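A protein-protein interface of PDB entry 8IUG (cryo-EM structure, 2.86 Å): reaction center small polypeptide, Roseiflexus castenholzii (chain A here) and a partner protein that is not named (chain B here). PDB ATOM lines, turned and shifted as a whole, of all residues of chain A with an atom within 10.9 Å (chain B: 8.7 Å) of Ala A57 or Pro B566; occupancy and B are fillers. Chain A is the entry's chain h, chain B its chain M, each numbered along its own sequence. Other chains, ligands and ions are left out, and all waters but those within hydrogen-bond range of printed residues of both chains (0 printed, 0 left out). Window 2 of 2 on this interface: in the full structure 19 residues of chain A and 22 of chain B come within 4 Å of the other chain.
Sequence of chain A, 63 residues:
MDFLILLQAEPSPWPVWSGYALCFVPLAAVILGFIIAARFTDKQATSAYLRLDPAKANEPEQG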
ATOM      1  N   LEU A  50      27.584  -0.169  11.444  1.00  0.00           N
ATOM      2  CA  LEU A  50      26.332   0.328  11.996  1.00  0.00           C
ATOM      3  C   LEU A  50      25.143  -0.195  11.207  1.00  0.00           C
ATOM      4  O   LEU A  50      25.041   0.026   9.998  1.00  0.00           O
ATOM      5  CB  LEU A  50      26.329   1.854  11.996  1.00  0.00           C
ATOM      6  CG  LEU A  50      27.230   2.573  12.995  1.00  0.00           C
ATOM      7  CD1 LEU A  50      27.242   4.056  12.699  1.00  0.00           C
ATOM      8  CD2 LEU A  50      26.755   2.319  14.409  1.00  0.00           C
ATOM      9  N   ARG A  51      24.241  -0.880  11.901  1.00  0.00           N
ATOM     10  CA  ARG A  51      22.998  -1.371  11.328  1.00  0.00           C
ATOM     11  C   ARG A  51      21.878  -1.106  12.319  1.00  0.00           C
ATOM     12  O   ARG A  51      22.110  -0.981  13.523  1.00  0.00           O
ATOM     13  CB  ARG A  51      23.069  -2.870  11.003  1.00  0.00           C
ATOM     14  CG  ARG A  51      24.066  -3.255   9.924  1.00  0.00           C
ATOM     15  CD  ARG A  51      24.161  -4.766   9.800  1.00  0.00           C
ATOM     16  NE  ARG A  51      24.903  -5.195   8.620  1.00  0.00           N
ATOM     17  CZ  ARG A  51      26.152  -5.637   8.632  1.00  0.00           C
ATOM     18  NH1 ARG A  51      26.849  -5.706   9.752  1.00  0.00           N
ATOM     19  NH2 ARG A  51      26.715  -6.023   7.495  1.00  0.00           N
ATOM     20  N   LEU A  52      20.657  -1.009  11.804  1.00  0.00           N
ATOM     21  CA  LEU A  52      19.484  -0.957  12.664  1.00  0.00           C
ATOM     22  C   LEU A  52      19.111  -2.368  13.098  1.00  0.00           C
ATOM     23  O   LEU A  52      19.134  -3.304  12.295  1.00  0.00           O
ATOM     24  CB  LEU A  52      18.309  -0.301  11.942  1.00  0.00           C
ATOM     25  CG  LEU A  52      18.508   1.106  11.374  1.00  0.00           C
ATOM     26  CD1 LEU A  52      17.237   1.589  10.713  1.00  0.00           C
ATOM     27  CD2 LEU A  52      18.939   2.071  12.453  1.00  0.00           C
ATOM     28  N   ASP A  53      18.771  -2.518  14.370  1.00  0.00           N
ATOM     29  CA  ASP A  53      18.510  -3.840  14.937  1.00  0.00           C
ATOM     30  C   ASP A  53      17.291  -4.463  14.269  1.00  0.00           C
ATOM     31  O   ASP A  53      16.221  -3.842  14.259  1.00  0.00           O
ATOM     32  CB  ASP A  53      18.294  -3.726  16.444  1.00  0.00           C
ATOM     33  CG  ASP A  53      18.650  -5.000  17.187  1.00  0.00           C
ATOM     34  OD1 ASP A  53      18.401  -6.099  16.656  1.00  0.00           O
ATOM     35  OD2 ASP A  53      19.184  -4.900  18.309  1.00  0.00           O
ATOM     36  N   PRO A  54      17.402  -5.664  13.694  1.00  0.00           N
ATOM     37  CA  PRO A  54      16.243  -6.251  13.002  1.00  0.00           C
ATOM     38  C   PRO A  54      15.042  -6.489  13.899  1.00  0.00           C
ATOM     39  O   PRO A  54      13.907  -6.465  13.411  1.00  0.00           O
ATOM     40  CB  PRO A  54      16.802  -7.566  12.439  1.00  0.00           C
ATOM     41  CG  PRO A  54      18.046  -7.829  13.206  1.00  0.00           C
ATOM     42  CD  PRO A  54      18.606  -6.497  13.551  1.00  0.00           C
ATOM     43  N   ALA A  55      15.253  -6.727  15.194  1.00  0.00           N
ATOM     44  CA  ALA A  55      14.135  -7.016  16.085  1.00  0.00           C
ATOM     45  C   ALA A  55      13.256  -5.788  16.290  1.00  0.00           C
ATOM     46  O   ALA A  55      12.026  -5.867  16.189  1.00  0.00           O
ATOM     47  CB  ALA A  55      14.654  -7.536  17.424  1.00  0.00           C
ATOM     48  N   LYS A  56      13.868  -4.640  16.580  1.00  0.00           N
ATOM     49  CA  LYS A  56      13.099  -3.426  16.828  1.00  0.00           C
ATOM     50  C   LYS A  56      12.573  -2.813  15.538  1.00  0.00           C
ATOM     51  O   LYS A  56      11.465  -2.267  15.514  1.00  0.00           O
ATOM     52  CB  LYS A  56      13.958  -2.409  17.578  1.00  0.00           C
ATOM     53  CG  LYS A  56      13.955  -2.578  19.083  1.00  0.00           C
ATOM     54  CD  LYS A  56      15.181  -1.928  19.702  1.00  0.00           C
ATOM     55  CE  LYS A  56      16.459  -2.418  19.047  1.00  0.00           C
ATOM     56  NZ  LYS A  56      16.383  -3.861  18.694  1.00  0.00           N
ATOM     57  N   ALA A  57      13.358  -2.881  14.460  1.00  0.00           N
ATOM     58  CA  ALA A  57      12.977  -2.222  13.216  1.00  0.00           C
ATOM     59  C   ALA A  57      11.752  -2.873  12.585  1.00  0.00           C
ATOM     60  O   ALA A  57      10.887  -2.178  12.040  1.00  0.00           O
ATOM     61  CB  ALA A  57      14.153  -2.229  12.243  1.00  0.00           C
ATOM     62  N   ASN A  58      11.662  -4.195  12.633  1.00  0.00           N
ATOM     63  CA  ASN A  58      10.515  -4.895  12.069  1.00  0.00           C
ATOM     64  C   ASN A  58       9.393  -5.018  13.095  1.00  0.00           C
ATOM     65  O   ASN A  58       8.224  -4.806  12.777  1.00  0.00           O
ATOM     66  CB  ASN A  58      10.920  -6.281  11.565  1.00  0.00           C
ATOM     67  CG  ASN A  58      11.798  -6.216  10.336  1.00  0.00           C
ATOM     68  OD1 ASN A  58      11.306  -6.135   9.213  1.00  0.00           O
ATOM     69  ND2 ASN A  58      13.108  -6.255  10.543  1.00  0.00           N
ATOM     70  N   THR B 549      12.290  -3.787  -2.553  1.00  0.00           N
ATOM     71  CA  THR B 549      12.481  -3.579  -1.123  1.00  0.00           C
ATOM     72  C   THR B 549      12.106  -2.167  -0.684  1.00  0.00           C
ATOM     73  O   THR B 549      12.500  -1.737   0.401  1.00  0.00           O
ATOM     74  CB  THR B 549      13.928  -3.884  -0.732  1.00  0.00           C
ATOM     75  OG1 THR B 549      14.809  -3.454  -1.774  1.00  0.00           O
ATOM     76  CG2 THR B 549      14.128  -5.353  -0.504  1.00  0.00           C
ATOM     77  N   SER B 550      11.346  -1.438  -1.504  1.00  0.00           N
ATOM     78  CA  SER B 550      11.074  -0.029  -1.240  1.00  0.00           C
ATOM     79  C   SER B 550      10.039   0.186  -0.147  1.00  0.00           C
ATOM     80  O   SER B 550       9.805   1.335   0.239  1.00  0.00           O
ATOM     81  CB  SER B 550      10.613   0.668  -2.519  1.00  0.00           C
ATOM     82  OG  SER B 550       9.346   0.194  -2.932  1.00  0.00           O
ATOM     83  N   LYS B 551       9.404  -0.878   0.346  1.00  0.00           N
ATOM     84  CA  LYS B 551       8.457  -0.738   1.446  1.00  0.00           C
ATOM     85  C   LYS B 551       9.144  -0.256   2.716  1.00  0.00           C
ATOM     86  O   LYS B 551       8.511   0.390   3.558  1.00  0.00           O
ATOM     87  CB  LYS B 551       7.751  -2.071   1.687  1.00  0.00           C
ATOM     88  CG  LYS B 551       6.750  -2.066   2.818  1.00  0.00           C
ATOM     89  CD  LYS B 551       5.911  -3.323   2.796  1.00  0.00           C
ATOM     90  CE  LYS B 551       5.775  -3.908   4.178  1.00  0.00           C
ATOM     91  NZ  LYS B 551       6.183  -2.931   5.221  1.00  0.00           N
ATOM     92  N   TRP B 552      10.434  -0.550   2.870  1.00  0.00           N
ATOM     93  CA  TRP B 552      11.211  -0.143   4.031  1.00  0.00           C
ATOM     94  C   TRP B 552      12.192   0.977   3.694  1.00  0.00           C
ATOM     95  O   TRP B 552      13.249   1.091   4.317  1.00  0.00           O
ATOM     96  CB  TRP B 552      11.948  -1.340   4.626  1.00  0.00           C
ATOM     97  CG  TRP B 552      11.048  -2.503   4.921  1.00  0.00           C
ATOM     98  CD1 TRP B 552      10.366  -2.742   6.073  1.00  0.00           C
ATOM     99  CD2 TRP B 552      10.731  -3.585   4.038  1.00  0.00           C
ATOM    100  NE1 TRP B 552       9.644  -3.900   5.965  1.00  0.00           N
ATOM    101  CE2 TRP B 552       9.852  -4.436   4.724  1.00  0.00           C
ATOM    102  CE3 TRP B 552      11.107  -3.913   2.734  1.00  0.00           C
ATOM    103  CZ2 TRP B 552       9.343  -5.593   4.150  1.00  0.00           C
ATOM    104  CZ3 TRP B 552      10.602  -5.056   2.171  1.00  0.00           C
ATOM    105  CH2 TRP B 552       9.732  -5.885   2.875  1.00  0.00           C
ATOM    106  N   LYS B 553      11.852   1.796   2.697  1.00  0.00           N
ATOM    107  CA  LYS B 553      12.584   3.023   2.371  1.00  0.00           C
ATOM    108  C   LYS B 553      14.045   2.750   2.028  1.00  0.00           C
ATOM    109  O   LYS B 553      14.949   3.449   2.489  1.00  0.00           O
ATOM    110  CB  LYS B 553      12.478   4.036   3.509  1.00  0.00           C
ATOM    111  CG  LYS B 553      11.087   4.167   4.093  1.00  0.00           C
ATOM    112  CD  LYS B 553      10.074   4.553   3.036  1.00  0.00           C
ATOM    113  CE  LYS B 553      10.410   5.904   2.437  1.00  0.00           C
ATOM    114  NZ  LYS B 553      11.165   6.758   3.395  1.00  0.00           N
ATOM    115  N   SER B 554      14.285   1.732   1.204  1.00  0.00           N
ATOM    116  CA  SER B 554      15.645   1.382   0.820  1.00  0.00           C
ATOM    117  C   SER B 554      16.226   2.317  -0.230  1.00  0.00           C
ATOM    118  O   SER B 554      17.445   2.326  -0.421  1.00  0.00           O
ATOM    119  CB  SER B 554      15.690  -0.052   0.300  1.00  0.00           C
ATOM    120  OG  SER B 554      14.826  -0.212  -0.805  1.00  0.00           O
ATOM    121  N   GLU B 560      21.182   5.443   4.040  1.00  0.00           N
ATOM    122  CA  GLU B 560      21.524   4.036   4.182  1.00  0.00           C
ATOM    123  C   GLU B 560      23.024   3.796   4.209  1.00  0.00           C
ATOM    124  O   GLU B 560      23.450   2.696   4.569  1.00  0.00           O
ATOM    125  CB  GLU B 560      20.899   3.220   3.048  1.00  0.00           C
ATOM    126  CG  GLU B 560      19.383   3.199   3.051  1.00  0.00           C
ATOM    127  CD  GLU B 560      18.806   2.331   4.152  1.00  0.00           C
ATOM    128  OE1 GLU B 560      18.589   2.842   5.267  1.00  0.00           O
ATOM    129  OE2 GLU B 560      18.563   1.133   3.902  1.00  0.00           O
ATOM    130  N   ALA B 563      23.663   3.973   8.258  1.00  0.00           N
ATOM    131  CA  ALA B 563      23.156   2.838   9.020  1.00  0.00           C
ATOM    132  C   ALA B 563      22.095   2.151   8.177  1.00  0.00           C
ATOM    133  O   ALA B 563      21.175   2.813   7.691  1.00  0.00           O
ATOM    134  CB  ALA B 563      22.573   3.278  10.364  1.00  0.00           C
ATOM    135  N   GLU B 564      22.213   0.838   8.012  1.00  0.00           N
ATOM    136  CA  GLU B 564      21.377   0.090   7.082  1.00  0.00           C
ATOM    137  C   GLU B 564      20.202  -0.556   7.804  1.00  0.00           C
ATOM    138  O   GLU B 564      20.384  -1.217   8.829  1.00  0.00           O
ATOM    139  CB  GLU B 564      22.198  -0.971   6.353  1.00  0.00           C
ATOM    140  CG  GLU B 564      23.540  -0.457   5.883  1.00  0.00           C
ATOM    141  CD  GLU B 564      23.946  -1.008   4.540  1.00  0.00           C
ATOM    142  OE1 GLU B 564      24.156  -2.231   4.440  1.00  0.00           O
ATOM    143  OE2 GLU B 564      24.063  -0.217   3.584  1.00  0.00           O
ATOM    144  N   GLY B 565      19.005  -0.371   7.254  1.00  0.00           N
ATOM    145  CA  GLY B 565      17.795  -0.889   7.842  1.00  0.00           C
ATOM    146  C   GLY B 565      17.261  -2.106   7.117  1.00  0.00           C
ATOM    147  O   GLY B 565      17.954  -2.729   6.309  1.00  0.00           O
ATOM    148  N   PRO B 566      16.004  -2.460   7.393  1.00  0.00           N
ATOM    149  CA  PRO B 566      15.463  -3.737   6.894  1.00  0.00           C
ATOM    150  C   PRO B 566      15.482  -3.904   5.383  1.00  0.00           C
ATOM    151  O   PRO B 566      15.670  -5.029   4.906  1.00  0.00           O
ATOM    152  CB  PRO B 566      14.030  -3.730   7.438  1.00  0.00           C
ATOM    153  CG  PRO B 566      14.115  -2.906   8.662  1.00  0.00           C
ATOM    154  CD  PRO B 566      15.096  -1.820   8.355  1.00  0.00           C
ATOM    155  N   GLY B 567      15.285  -2.834   4.612  1.00  0.00           N
ATOM    156  CA  GLY B 567      15.287  -2.974   3.164  1.00  0.00           C
ATOM    157  C   GLY B 567      16.634  -3.402   2.615  1.00  0.00           C
ATOM    158  O   GLY B 567      16.725  -4.320   1.795  1.00  0.00           O
ATOM    159  N   THR B 568      17.705  -2.751   3.071  1.00  0.00           N
ATOM    160  CA  THR B 568      19.037  -3.101   2.589  1.00  0.00           C
ATOM    161  C   THR B 568      19.452  -4.483   3.076  1.00  0.00           C
ATOM    162  O   THR B 568      20.107  -5.236   2.344  1.00  0.00           O
ATOM    163  CB  THR B 568      20.052  -2.050   3.027  1.00  0.00           C
ATOM    164  OG1 THR B 568      19.508  -0.746   2.810  1.00  0.00           O
ATOM    165  CG2 THR B 568      21.323  -2.180   2.218  1.00  0.00           C
ATOM    166  N   GLN B 569      19.077  -4.834   4.306  1.00  0.00           N
ATOM    167  CA  GLN B 569      19.358  -6.171   4.815  1.00  0.00           C
ATOM    168  C   GLN B 569      18.667  -7.236   3.974  1.00  0.00           C
ATOM    169  O   GLN B 569      19.268  -8.266   3.646  1.00  0.00           O
ATOM    170  CB  GLN B 569      18.929  -6.266   6.277  1.00  0.00           C
ATOM    171  CG  GLN B 569      19.620  -5.264   7.190  1.00  0.00           C
ATOM    172  CD  GLN B 569      19.043  -5.253   8.588  1.00  0.00           C
ATOM    173  OE1 GLN B 569      18.082  -5.958   8.875  1.00  0.00           O
ATOM    174  NE2 GLN B 569      19.621  -4.447   9.462  1.00  0.00           N
ATOM    175  N   ARG B 570      17.409  -6.997   3.597  1.00  0.00           N
ATOM    176  CA  ARG B 570      16.693  -7.949   2.755  1.00  0.00           C
ATOM    177  C   ARG B 570      17.305  -8.049   1.362  1.00  0.00           C
ATOM    178  O   ARG B 570      17.373  -9.141   0.793  1.00  0.00           O
ATOM    179  CB  ARG B 570      15.219  -7.567   2.666  1.00  0.00           C
ATOM    180  CG  ARG B 570      14.400  -8.008   3.855  1.00  0.00           C
ATOM    181  CD  ARG B 570      12.944  -7.675   3.650  1.00  0.00           C
ATOM    182  NE  ARG B 570      12.082  -8.271   4.663  1.00  0.00           N
ATOM    183  CZ  ARG B 570      11.806  -7.716   5.835  1.00  0.00           C
ATOM    184  NH1 ARG B 570      12.343  -6.567   6.198  1.00  0.00           N
ATOM    185  NH2 ARG B 570      10.968  -8.332   6.661  1.00  0.00           N
ATOM    186  N   ALA B 571      17.742  -6.926   0.787  1.00  0.00           N
ATOM    187  CA  ALA B 571      18.393  -6.981  -0.523  1.00  0.00           C
ATOM    188  C   ALA B 571      19.690  -7.783  -0.472  1.00  0.00           C
ATOM    189  O   ALA B 571      19.963  -8.619  -1.353  1.00  0.00           O
ATOM    190  CB  ALA B 571      18.659  -5.567  -1.032  1.00  0.00           C
ATOM    191  N   GLN B 572      20.496  -7.551   0.566  1.00  0.00           N
ATOM    192  CA  GLN B 572      21.726  -8.311   0.745  1.00  0.00           C
ATOM    193  C   GLN B 572      21.439  -9.796   0.890  1.00  0.00           C
ATOM    194  O   GLN B 572      22.110 -10.630   0.271  1.00  0.00           O
ATOM    195  CB  GLN B 572      22.480  -7.795   1.967  1.00  0.00           C
ATOM    196  CG  GLN B 572      23.164  -6.468   1.768  1.00  0.00           C
ATOM    197  CD  GLN B 572      24.045  -6.103   2.935  1.00  0.00           C
ATOM    198  OE1 GLN B 572      23.688  -6.326   4.087  1.00  0.00           O
ATOM    199  NE2 GLN B 572      25.209  -5.548   2.644  1.00  0.00           N
ATOM    200  N   LEU B 573      20.445 -10.150   1.708  1.00  0.00           N
ATOM    201  CA  LEU B 573      20.122 -11.560   1.909  1.00  0.00           C
ATOM    202  C   LEU B 573      19.605 -12.205   0.632  1.00  0.00           C
ATOM    203  O   LEU B 573      19.939 -13.357   0.339  1.00  0.00           O
ATOM    204  CB  LEU B 573      19.109 -11.714   3.038  1.00  0.00           C
ATOM    205  CG  LEU B 573      19.667 -11.478   4.438  1.00  0.00           C
ATOM    206  CD1 LEU B 573      18.618 -11.769   5.469  1.00  0.00           C
ATOM    207  CD2 LEU B 573      20.885 -12.341   4.669  1.00  0.00           C
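Ala B563 touches Leu A50.
N of Glu B564 touches O of Leu A50 (3.5 Å).
Arg A51 touches Glu B564.
Gly B565 touches Leu A52.
CG of Pro B566 touches CB of Ala A57 (3.6 Å).
Pro B566 touches Asn A58.
Ala A57 touches just one residue of chain B: Pro B566 (3.6 Å).
Pro B566 touches two residues of chain A.
No residue of chain A comes within 4 Å of Gly B567.
Arg B570 touches just one residue of chain A: Asn A58.
Of the printed residues of chain A, Glu B564 touches Leu A50, Arg A51 and Leu A52.
Of the printed residues of chain B, Leu A50 touches Ala B563 (3.5 Å) and Glu B564 (3.5 Å).
Printed residues of chain B within 4 Å of Leu A52: Glu B564 (3.0 Å), Gly B565 (3.8 Å) and Gln B569 (3.1 Å).
The nearest residue of chain A that does not touch Pro B566 is Leu A52 (4.7 Å).
The backbone carbonyl oxygen of Glu B564 is in hydrogen-bond range of the backbone NH of Leu A52 (3.0 Å).
The backbone carbonyl oxygen (O) of Leu A52 is in hydrogen-bond range of the side-chain amide nitrogen (NE2) of Gln B569, 3.1 Å away.
NH1 of Arg B570 lies within hydrogen-bond range of OD1 of Asn A58 (3.2 Å).
Printed residues of chain B that touch a printed residue of chain A: Ala B563, Glu B564, Gly B565, Pro B566, Gln B569 and Arg B570.
Of the 9 printed residues of chain A, 5 touch a printed residue of chain B.
Hydrophobic or aromatic side chains of chain A that line the printed part of chain B: Leu A52 and Ala A57.
O of Glu B564 is in hydrogen-bond range of NE2 of Gln B569 (3.4 Å).
The backbone carbonyl oxygen of Pro A54 is in hydrogen-bond range of the side-chain amide nitrogen of Asn A58 (3.0 Å).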
